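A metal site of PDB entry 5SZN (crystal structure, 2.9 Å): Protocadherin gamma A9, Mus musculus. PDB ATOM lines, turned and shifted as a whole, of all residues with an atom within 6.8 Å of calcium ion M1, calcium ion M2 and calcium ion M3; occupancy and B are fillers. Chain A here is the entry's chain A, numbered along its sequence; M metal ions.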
ATOM      1  N   GLU A 225      34.824  22.833 -26.794  1.00  0.00           N
ATOM      2  CA  GLU A 225      35.738  21.746 -26.484  1.00  0.00           C
ATOM      3  C   GLU A 225      35.806  20.704 -27.595  1.00  0.00           C
ATOM      4  O   GLU A 225      36.828  20.019 -27.735  1.00  0.00           O
ATOM      5  CB  GLU A 225      35.330  21.072 -25.161  1.00  0.00           C
ATOM      6  CG  GLU A 225      33.873  20.638 -25.093  1.00  0.00           C
ATOM      7  CD  GLU A 225      33.534  19.928 -23.800  1.00  0.00           C
ATOM      8  OE1 GLU A 225      34.457  19.407 -23.147  1.00  0.00           O
ATOM      9  OE2 GLU A 225      32.337  19.898 -23.428  1.00  0.00           O
ATOM     10  N   ASN A 226      34.751  20.579 -28.402  1.00  0.00           N
ATOM     11  CA  ASN A 226      34.711  19.610 -29.481  1.00  0.00           C
ATOM     12  C   ASN A 226      35.565  20.051 -30.657  1.00  0.00           C
ATOM     13  O   ASN A 226      35.384  19.579 -31.789  1.00  0.00           O
ATOM     14  CB  ASN A 226      33.269  19.385 -29.928  1.00  0.00           C
ATOM     15  CG  ASN A 226      32.558  20.689 -30.275  1.00  0.00           C
ATOM     16  OD1 ASN A 226      33.194  21.716 -30.491  1.00  0.00           O
ATOM     17  ND2 ASN A 226      31.237  20.630 -30.342  1.00  0.00           N
ATOM     18  N   LEU A 279      40.596  19.037 -26.995  1.00  0.00           N
ATOM     19  CA  LEU A 279      40.423  19.729 -25.727  1.00  0.00           C
ATOM     20  C   LEU A 279      39.233  19.152 -24.960  1.00  0.00           C
ATOM     21  O   LEU A 279      38.419  18.403 -25.488  1.00  0.00           O
ATOM     22  CB  LEU A 279      40.242  21.228 -25.941  1.00  0.00           C
ATOM     23  CG  LEU A 279      41.443  21.968 -26.525  1.00  0.00           C
ATOM     24  CD1 LEU A 279      41.153  23.453 -26.666  1.00  0.00           C
ATOM     25  CD2 LEU A 279      42.683  21.740 -25.658  1.00  0.00           C
ATOM     26  N   ASP A 280      39.152  19.539 -23.689  1.00  0.00           N
ATOM     27  CA  ASP A 280      38.091  19.041 -22.806  1.00  0.00           C
ATOM     28  C   ASP A 280      37.783  20.108 -21.767  1.00  0.00           C
ATOM     29  O   ASP A 280      38.652  20.487 -20.980  1.00  0.00           O
ATOM     30  CB  ASP A 280      38.521  17.745 -22.129  1.00  0.00           C
ATOM     31  CG  ASP A 280      37.349  16.987 -21.541  1.00  0.00           C
ATOM     32  OD1 ASP A 280      36.252  17.045 -22.120  1.00  0.00           O
ATOM     33  OD2 ASP A 280      37.539  16.327 -20.497  1.00  0.00           O
ATOM     34  N   TYR A 281      36.530  20.592 -21.770  1.00  0.00           N
ATOM     35  CA  TYR A 281      36.124  21.615 -20.812  1.00  0.00           C
ATOM     36  C   TYR A 281      36.269  21.138 -19.377  1.00  0.00           C
ATOM     37  O   TYR A 281      36.560  21.945 -18.486  1.00  0.00           O
ATOM     38  CB  TYR A 281      34.679  22.034 -21.092  1.00  0.00           C
ATOM     39  CG  TYR A 281      34.147  23.134 -20.181  1.00  0.00           C
ATOM     40  CD1 TYR A 281      34.293  24.472 -20.530  1.00  0.00           C
ATOM     41  CD2 TYR A 281      33.493  22.831 -19.002  1.00  0.00           C
ATOM     42  CE1 TYR A 281      33.817  25.479 -19.710  1.00  0.00           C
ATOM     43  CE2 TYR A 281      33.004  23.828 -18.182  1.00  0.00           C
ATOM     44  CZ  TYR A 281      33.167  25.146 -18.543  1.00  0.00           C
ATOM     45  OH  TYR A 281      32.691  26.144 -17.722  1.00  0.00           O
ATOM     46  N   GLU A 282      36.081  19.850 -19.133  1.00  0.00           N
ATOM     47  CA  GLU A 282      36.148  19.330 -17.771  1.00  0.00           C
ATOM     48  C   GLU A 282      37.584  19.196 -17.282  1.00  0.00           C
ATOM     49  O   GLU A 282      37.838  19.306 -16.082  1.00  0.00           O
ATOM     50  CB  GLU A 282      35.434  17.976 -17.682  1.00  0.00           C
ATOM     51  CG  GLU A 282      33.932  18.052 -17.917  1.00  0.00           C
ATOM     52  CD  GLU A 282      33.561  18.216 -19.375  1.00  0.00           C
ATOM     53  OE1 GLU A 282      34.413  17.952 -20.245  1.00  0.00           O
ATOM     54  OE2 GLU A 282      32.410  18.611 -19.657  1.00  0.00           O
ATOM     55  N   GLU A 310      34.548  26.412 -23.824  1.00  0.00           N
ATOM     56  CA  GLU A 310      33.195  26.378 -23.312  1.00  0.00           C
ATOM     57  C   GLU A 310      32.646  24.955 -23.415  1.00  0.00           C
ATOM     58  O   GLU A 310      33.061  24.181 -24.281  1.00  0.00           O
ATOM     59  CB  GLU A 310      32.278  27.356 -24.049  1.00  0.00           C
ATOM     60  CG  GLU A 310      32.700  28.811 -23.906  1.00  0.00           C
ATOM     61  CD  GLU A 310      32.585  29.316 -22.474  1.00  0.00           C
ATOM     62  OE1 GLU A 310      31.457  29.481 -21.989  1.00  0.00           O
ATOM     63  OE2 GLU A 310      33.641  29.540 -21.844  1.00  0.00           O
ATOM     64  N   ASP A 311      31.712  24.629 -22.535  1.00  0.00           N
ATOM     65  CA  ASP A 311      31.239  23.259 -22.403  1.00  0.00           C
ATOM     66  C   ASP A 311      30.348  22.864 -23.574  1.00  0.00           C
ATOM     67  O   ASP A 311      29.680  23.701 -24.188  1.00  0.00           O
ATOM     68  CB  ASP A 311      30.494  23.089 -21.081  1.00  0.00           C
ATOM     69  CG  ASP A 311      29.972  21.678 -20.885  1.00  0.00           C
ATOM     70  OD1 ASP A 311      30.793  20.755 -20.718  1.00  0.00           O
ATOM     71  OD2 ASP A 311      28.730  21.499 -20.897  1.00  0.00           O
ATOM     72  N   VAL A 312      30.348  21.566 -23.886  1.00  0.00           N
ATOM     73  CA  VAL A 312      29.523  21.003 -24.944  1.00  0.00           C
ATOM     74  C   VAL A 312      28.901  19.715 -24.420  1.00  0.00           C
ATOM     75  O   VAL A 312      29.533  18.964 -23.664  1.00  0.00           O
ATOM     76  CB  VAL A 312      30.334  20.738 -26.236  1.00  0.00           C
ATOM     77  CG1 VAL A 312      29.485  20.052 -27.294  1.00  0.00           C
ATOM     78  CG2 VAL A 312      30.885  22.038 -26.778  1.00  0.00           C
ATOM     79  N   ASN A 313      27.643  19.460 -24.798  1.00  0.00           N
ATOM     80  CA  ASN A 313      26.967  18.229 -24.423  1.00  0.00           C
ATOM     81  C   ASN A 313      27.583  17.011 -25.109  1.00  0.00           C
ATOM     82  O   ASN A 313      27.101  16.589 -26.155  1.00  0.00           O
ATOM     83  CB  ASN A 313      25.476  18.319 -24.750  1.00  0.00           C
ATOM     84  CG  ASN A 313      24.662  17.203 -24.120  1.00  0.00           C
ATOM     85  OD1 ASN A 313      25.101  16.580 -23.156  1.00  0.00           O
ATOM     86  ND2 ASN A 313      23.476  16.954 -24.657  1.00  0.00           N
ATOM     87  N   ASP A 314      28.654  16.458 -24.530  1.00  0.00           N
ATOM     88  CA  ASP A 314      29.302  15.254 -25.031  1.00  0.00           C
ATOM     89  C   ASP A 314      29.426  14.199 -23.953  1.00  0.00           C
ATOM     90  O   ASP A 314      30.335  13.360 -23.984  1.00  0.00           O
ATOM     91  CB  ASP A 314      30.670  15.576 -25.637  1.00  0.00           C
ATOM     92  CG  ASP A 314      31.666  16.062 -24.600  1.00  0.00           C
ATOM     93  OD1 ASP A 314      31.236  16.701 -23.621  1.00  0.00           O
ATOM     94  OD2 ASP A 314      32.884  15.815 -24.762  1.00  0.00           O
ATOM     95  N   ASN A 315      28.538  14.236 -22.964  1.00  0.00           N
ATOM     96  CA  ASN A 315      28.530  13.281 -21.864  1.00  0.00           C
ATOM     97  C   ASN A 315      27.099  12.885 -21.555  1.00  0.00           C
ATOM     98  O   ASN A 315      26.159  13.654 -21.769  1.00  0.00           O
ATOM     99  CB  ASN A 315      29.201  13.863 -20.618  1.00  0.00           C
ATOM    100  CG  ASN A 315      30.682  14.101 -20.801  1.00  0.00           C
ATOM    101  OD1 ASN A 315      31.496  13.211 -20.565  1.00  0.00           O
ATOM    102  ND2 ASN A 315      31.038  15.299 -21.249  1.00  0.00           N
ATOM    103  N   ARG A 316      26.936  11.637 -21.028  1.00  0.00           N
ATOM    104  CA  ARG A 316      25.664  11.026 -20.683  1.00  0.00           C
ATOM    105  C   ARG A 316      25.431  11.073 -19.174  1.00  0.00           C
ATOM    106  O   ARG A 316      26.378  11.066 -18.387  1.00  0.00           O
ATOM    107  CB  ARG A 316      25.622   9.573 -21.152  1.00  0.00           C
ATOM    108  CG  ARG A 316      25.181   9.401 -22.594  1.00  0.00           C
ATOM    109  CD  ARG A 316      25.026   7.927 -22.933  1.00  0.00           C
ATOM    110  NE  ARG A 316      24.365   7.736 -24.216  1.00  0.00           N
ATOM    111  CZ  ARG A 316      24.997   7.725 -25.385  1.00  0.00           C
ATOM    112  NH1 ARG A 316      26.306   7.906 -25.433  1.00  0.00           N
ATOM    113  NH2 ARG A 316      24.305   7.541 -26.507  1.00  0.00           N
ATOM    114  N   PRO A 317      24.166  11.131 -18.755  1.00  0.00           N
ATOM    115  CA  PRO A 317      23.864  11.118 -17.324  1.00  0.00           C
ATOM    116  C   PRO A 317      24.284   9.797 -16.688  1.00  0.00           C
ATOM    117  O   PRO A 317      24.285   8.750 -17.335  1.00  0.00           O
ATOM    118  CB  PRO A 317      22.350  11.311 -17.268  1.00  0.00           C
ATOM    119  CG  PRO A 317      21.995  11.929 -18.589  1.00  0.00           C
ATOM    120  CD  PRO A 317      22.960  11.346 -19.569  1.00  0.00           C
ATOM    121  N   ASP A 345      25.226  14.433 -13.959  1.00  0.00           N
ATOM    122  CA  ASP A 345      25.832  14.631 -15.269  1.00  0.00           C
ATOM    123  C   ASP A 345      27.182  15.333 -15.105  1.00  0.00           C
ATOM    124  O   ASP A 345      27.358  16.161 -14.207  1.00  0.00           O
ATOM    125  CB  ASP A 345      24.926  15.448 -16.194  1.00  0.00           C
ATOM    126  CG  ASP A 345      25.313  15.326 -17.655  1.00  0.00           C
ATOM    127  OD1 ASP A 345      26.521  15.290 -17.972  1.00  0.00           O
ATOM    128  OD2 ASP A 345      24.389  15.271 -18.507  1.00  0.00           O
ATOM    129  N   GLN A 346      28.128  14.976 -15.979  1.00  0.00           N
ATOM    130  CA  GLN A 346      29.441  15.607 -15.933  1.00  0.00           C
ATOM    131  C   GLN A 346      29.425  17.005 -16.535  1.00  0.00           C
ATOM    132  O   GLN A 346      30.215  17.854 -16.136  1.00  0.00           O
ATOM    133  CB  GLN A 346      30.462  14.742 -16.680  1.00  0.00           C
ATOM    134  CG  GLN A 346      30.537  13.302 -16.177  1.00  0.00           C
ATOM    135  CD  GLN A 346      31.542  12.474 -16.956  1.00  0.00           C
ATOM    136  OE1 GLN A 346      32.239  12.990 -17.840  1.00  0.00           O
ATOM    137  NE2 GLN A 346      31.627  11.195 -16.633  1.00  0.00           N
ATOM    138  N   ASP A 347      28.520  17.257 -17.476  1.00  0.00           N
ATOM    139  CA  ASP A 347      28.445  18.555 -18.133  1.00  0.00           C
ATOM    140  C   ASP A 347      27.914  19.618 -17.178  1.00  0.00           C
ATOM    141  O   ASP A 347      27.469  19.329 -16.065  1.00  0.00           O
ATOM    142  CB  ASP A 347      27.573  18.469 -19.378  1.00  0.00           C
ATOM    143  CG  ASP A 347      28.160  17.565 -20.446  1.00  0.00           C
ATOM    144  OD1 ASP A 347      29.399  17.543 -20.592  1.00  0.00           O
ATOM    145  OD2 ASP A 347      27.377  16.878 -21.146  1.00  0.00           O
ATOM    146  N   SER A 348      27.954  20.859 -17.633  1.00  0.00           N
ATOM    147  CA  SER A 348      27.509  22.008 -16.848  1.00  0.00           C
ATOM    148  C   SER A 348      26.313  22.664 -17.532  1.00  0.00           C
ATOM    149  O   SER A 348      26.040  22.443 -18.713  1.00  0.00           O
ATOM    150  CB  SER A 348      28.639  23.022 -16.680  1.00  0.00           C
ATOM    151  OG  SER A 348      29.811  22.414 -16.156  1.00  0.00           O
ATOM    152  N   LYS A 350      22.668  23.782 -18.820  1.00  0.00           N
ATOM    153  CA  LYS A 350      21.560  23.014 -19.392  1.00  0.00           C
ATOM    154  C   LYS A 350      22.001  21.643 -19.873  1.00  0.00           C
ATOM    155  O   LYS A 350      21.151  20.754 -20.026  1.00  0.00           O
ATOM    156  CB  LYS A 350      20.931  23.800 -20.548  1.00  0.00           C
ATOM    157  N   ASN A 351      23.291  21.447 -20.134  1.00  0.00           N
ATOM    158  CA  ASN A 351      23.811  20.124 -20.450  1.00  0.00           C
ATOM    159  C   ASN A 351      24.024  19.256 -19.222  1.00  0.00           C
ATOM    160  O   ASN A 351      24.268  18.051 -19.362  1.00  0.00           O
ATOM    161  CB  ASN A 351      25.127  20.258 -21.225  1.00  0.00           C
ATOM    162  CG  ASN A 351      24.994  21.069 -22.502  1.00  0.00           C
ATOM    163  OD1 ASN A 351      24.007  20.935 -23.233  1.00  0.00           O
ATOM    164  ND2 ASN A 351      25.984  21.912 -22.778  1.00  0.00           N
ATOM    165  N   GLY A 352      23.944  19.831 -18.019  1.00  0.00           N
ATOM    166  CA  GLY A 352      24.159  19.094 -16.798  1.00  0.00           C
ATOM    167  C   GLY A 352      22.887  18.791 -16.039  1.00  0.00           C
ATOM    168  O   GLY A 352      22.856  17.919 -15.172  1.00  0.00           O
ATOM    169  N   GLN A 353      21.807  19.522 -16.351  1.00  0.00           N
ATOM    170  CA  GLN A 353      20.519  19.249 -15.729  1.00  0.00           C
ATOM    171  C   GLN A 353      19.962  17.930 -16.243  1.00  0.00           C
ATOM    172  O   GLN A 353      20.039  17.617 -17.441  1.00  0.00           O
ATOM    173  CB  GLN A 353      19.535  20.382 -16.011  1.00  0.00           C
ATOM    174  CG  GLN A 353      19.952  21.714 -15.414  1.00  0.00           C
ATOM    175  CD  GLN A 353      18.929  22.804 -15.695  1.00  0.00           C
ATOM    176  OE1 GLN A 353      17.841  22.547 -16.183  1.00  0.00           O
ATOM    177  NE2 GLN A 353      19.299  24.043 -15.393  1.00  0.00           N
ATOM    178  N   ASP A 398      19.166  14.284 -20.350  1.00  0.00           N
ATOM    179  CA  ASP A 398      19.623  15.615 -19.978  1.00  0.00           C
ATOM    180  C   ASP A 398      18.812  16.674 -20.713  1.00  0.00           C
ATOM    181  O   ASP A 398      18.122  16.398 -21.702  1.00  0.00           O
ATOM    182  CB  ASP A 398      21.121  15.789 -20.234  1.00  0.00           C
ATOM    183  CG  ASP A 398      21.518  15.548 -21.686  1.00  0.00           C
ATOM    184  OD1 ASP A 398      20.649  15.545 -22.581  1.00  0.00           O
ATOM    185  OD2 ASP A 398      22.736  15.366 -21.938  1.00  0.00           O
ATOM    186  N   ARG A 399      18.902  17.910 -20.228  1.00  0.00           N
ATOM    187  CA  ARG A 399      18.126  19.015 -20.759  1.00  0.00           C
ATOM    188  C   ARG A 399      18.873  19.805 -21.834  1.00  0.00           C
ATOM    189  O   ARG A 399      18.363  20.837 -22.294  1.00  0.00           O
ATOM    190  CB  ARG A 399      17.697  19.947 -19.619  1.00  0.00           C
ATOM    191  CG  ARG A 399      16.334  20.599 -19.830  1.00  0.00           C
ATOM    192  CD  ARG A 399      16.022  21.580 -18.708  1.00  0.00           C
ATOM    193  NE  ARG A 399      15.870  20.927 -17.415  1.00  0.00           N
ATOM    194  CZ  ARG A 399      14.707  20.526 -16.912  1.00  0.00           C
ATOM    195  NH1 ARG A 399      13.584  20.695 -17.606  1.00  0.00           N
ATOM    196  NH2 ARG A 399      14.661  19.946 -15.724  1.00  0.00           N
ATOM    197  N   GLY A 400      20.053  19.347 -22.255  1.00  0.00           N
ATOM    198  CA  GLY A 400      20.825  20.043 -23.259  1.00  0.00           C
ATOM    199  C   GLY A 400      20.397  19.712 -24.677  1.00  0.00           C
ATOM    200  O   GLY A 400      19.423  18.988 -24.917  1.00  0.00           O
ATOM    201  N   MET A 404      21.022  13.760 -24.546  1.00  0.00           N
ATOM    202  CA  MET A 404      21.586  12.434 -24.348  1.00  0.00           C
ATOM    203  C   MET A 404      20.888  11.765 -23.185  1.00  0.00           C
ATOM    204  O   MET A 404      20.822  12.323 -22.087  1.00  0.00           O
ATOM    205  CB  MET A 404      23.095  12.502 -24.086  1.00  0.00           C
ATOM    206  CG  MET A 404      23.927  12.960 -25.272  1.00  0.00           C
ATOM    207  SD  MET A 404      25.697  12.773 -24.951  1.00  0.00           S
ATOM    208  CE  MET A 404      26.375  13.282 -26.531  1.00  0.00           C
HETATM  209 CA    CA M   1      31.456  18.353 -21.869  1.00  0.00          CA
HETATM  210 CA    CA M   2      34.069  16.741 -22.946  1.00  0.00          CA
HETATM  211 CA    CA M   3      25.356  16.007 -20.552  1.00  0.00          CA
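Five residues have an atom within 4 Å of calcium ion M2: Glu 225, Asp 280, Glu 282, Asp 314 and Asn 315.
The nearest printed residue that does not touch calcium ion M2 is Tyr 281 (4.7 Å).
The side-chain carboxylate (OD1) of Asp 280 is bound to calcium ion M2 (2.4 Å).
Calcium ion M2 is bound by the side-chain carboxylate (OD2) of Asp 314 (2.4 Å).
OE1 of Glu 225 is bound to calcium ion M2.
Slightly farther from calcium ion M2 lies OD1 of Asp 314 (2.9 Å).
Slightly farther from calcium ion M2 lies OE1 of Glu 282 (3.0 Å).
Six residues have an atom within 4 Å of calcium ion M3: Asn 313, Asn 315, Asp 345, Asp 347, Asn 351 and Asp 398.
The nearest printed residue that does not touch calcium ion M3 is Arg 316 (4.7 Å).
Calcium ion M3 is bound by OD2 of Asp 347 (2.3 Å), OD2 of Asp 345 (2.4 Å), O of Asn 351 (2.6 Å), OD1 of Asn 313 (2.7 Å) and O of Asn 315 (2.8 Å).
Slightly farther from calcium ion M3 lies OD1 of Asp 345 (2.9 Å).
Slightly farther from calcium ion M3 lies the side-chain carboxylate (OD2) of Asp 398 (3.0 Å).
The nearest printed residue that does not touch calcium ion M1 is Asn 313 (4.9 Å).
Calcium ion M1 is bound by the side-chain carboxylate of Glu 225 (2.4 Å), the side-chain carboxylate of Asp 314 (2.4 Å), the side-chain carboxylate of Glu 282 (2.4 Å), the side-chain carboxylate of Asp 347 (2.6 Å), the backbone carbonyl oxygen of Val 312 (2.7 Å) and the side-chain carboxylate of Asp 311 (2.7 Å).
Calcium ion M1 has six donor atoms within binding distance.
Slightly farther from calcium ion M1 lies the side-chain amide nitrogen (ND2) of Asn 315 (3.1 Å).
The side-chain carboxylate (OD1) of Asp 314 sits close to the side-chain amide nitrogen (ND2) of Asn 315 (2.8 Å).
OE1 of Glu 225 lies close to N of Tyr 281, 2.8 Å away.
ND2 of Asn 351 is in hydrogen-bond range of OD2 of Asp 311 (3.4 Å).
OD2 of Asp 398 sits at hydrogen-bond distance from ND2 of Asn 313 (3.2 Å).
OD2 of Asp 311 lies within hydrogen-bond range of N of Ser 348 (3.4 Å).
OD1 of Asn 315 lies close to OE1 of Gln 346, at 2.8 Å.
The backbone NH (N) of Asn 315 lies close to the side-chain sulfur (SD) of Met 404 (3.8 Å).
OD1 of Asp 398 sits at hydrogen-bond distance from N of Met 404.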
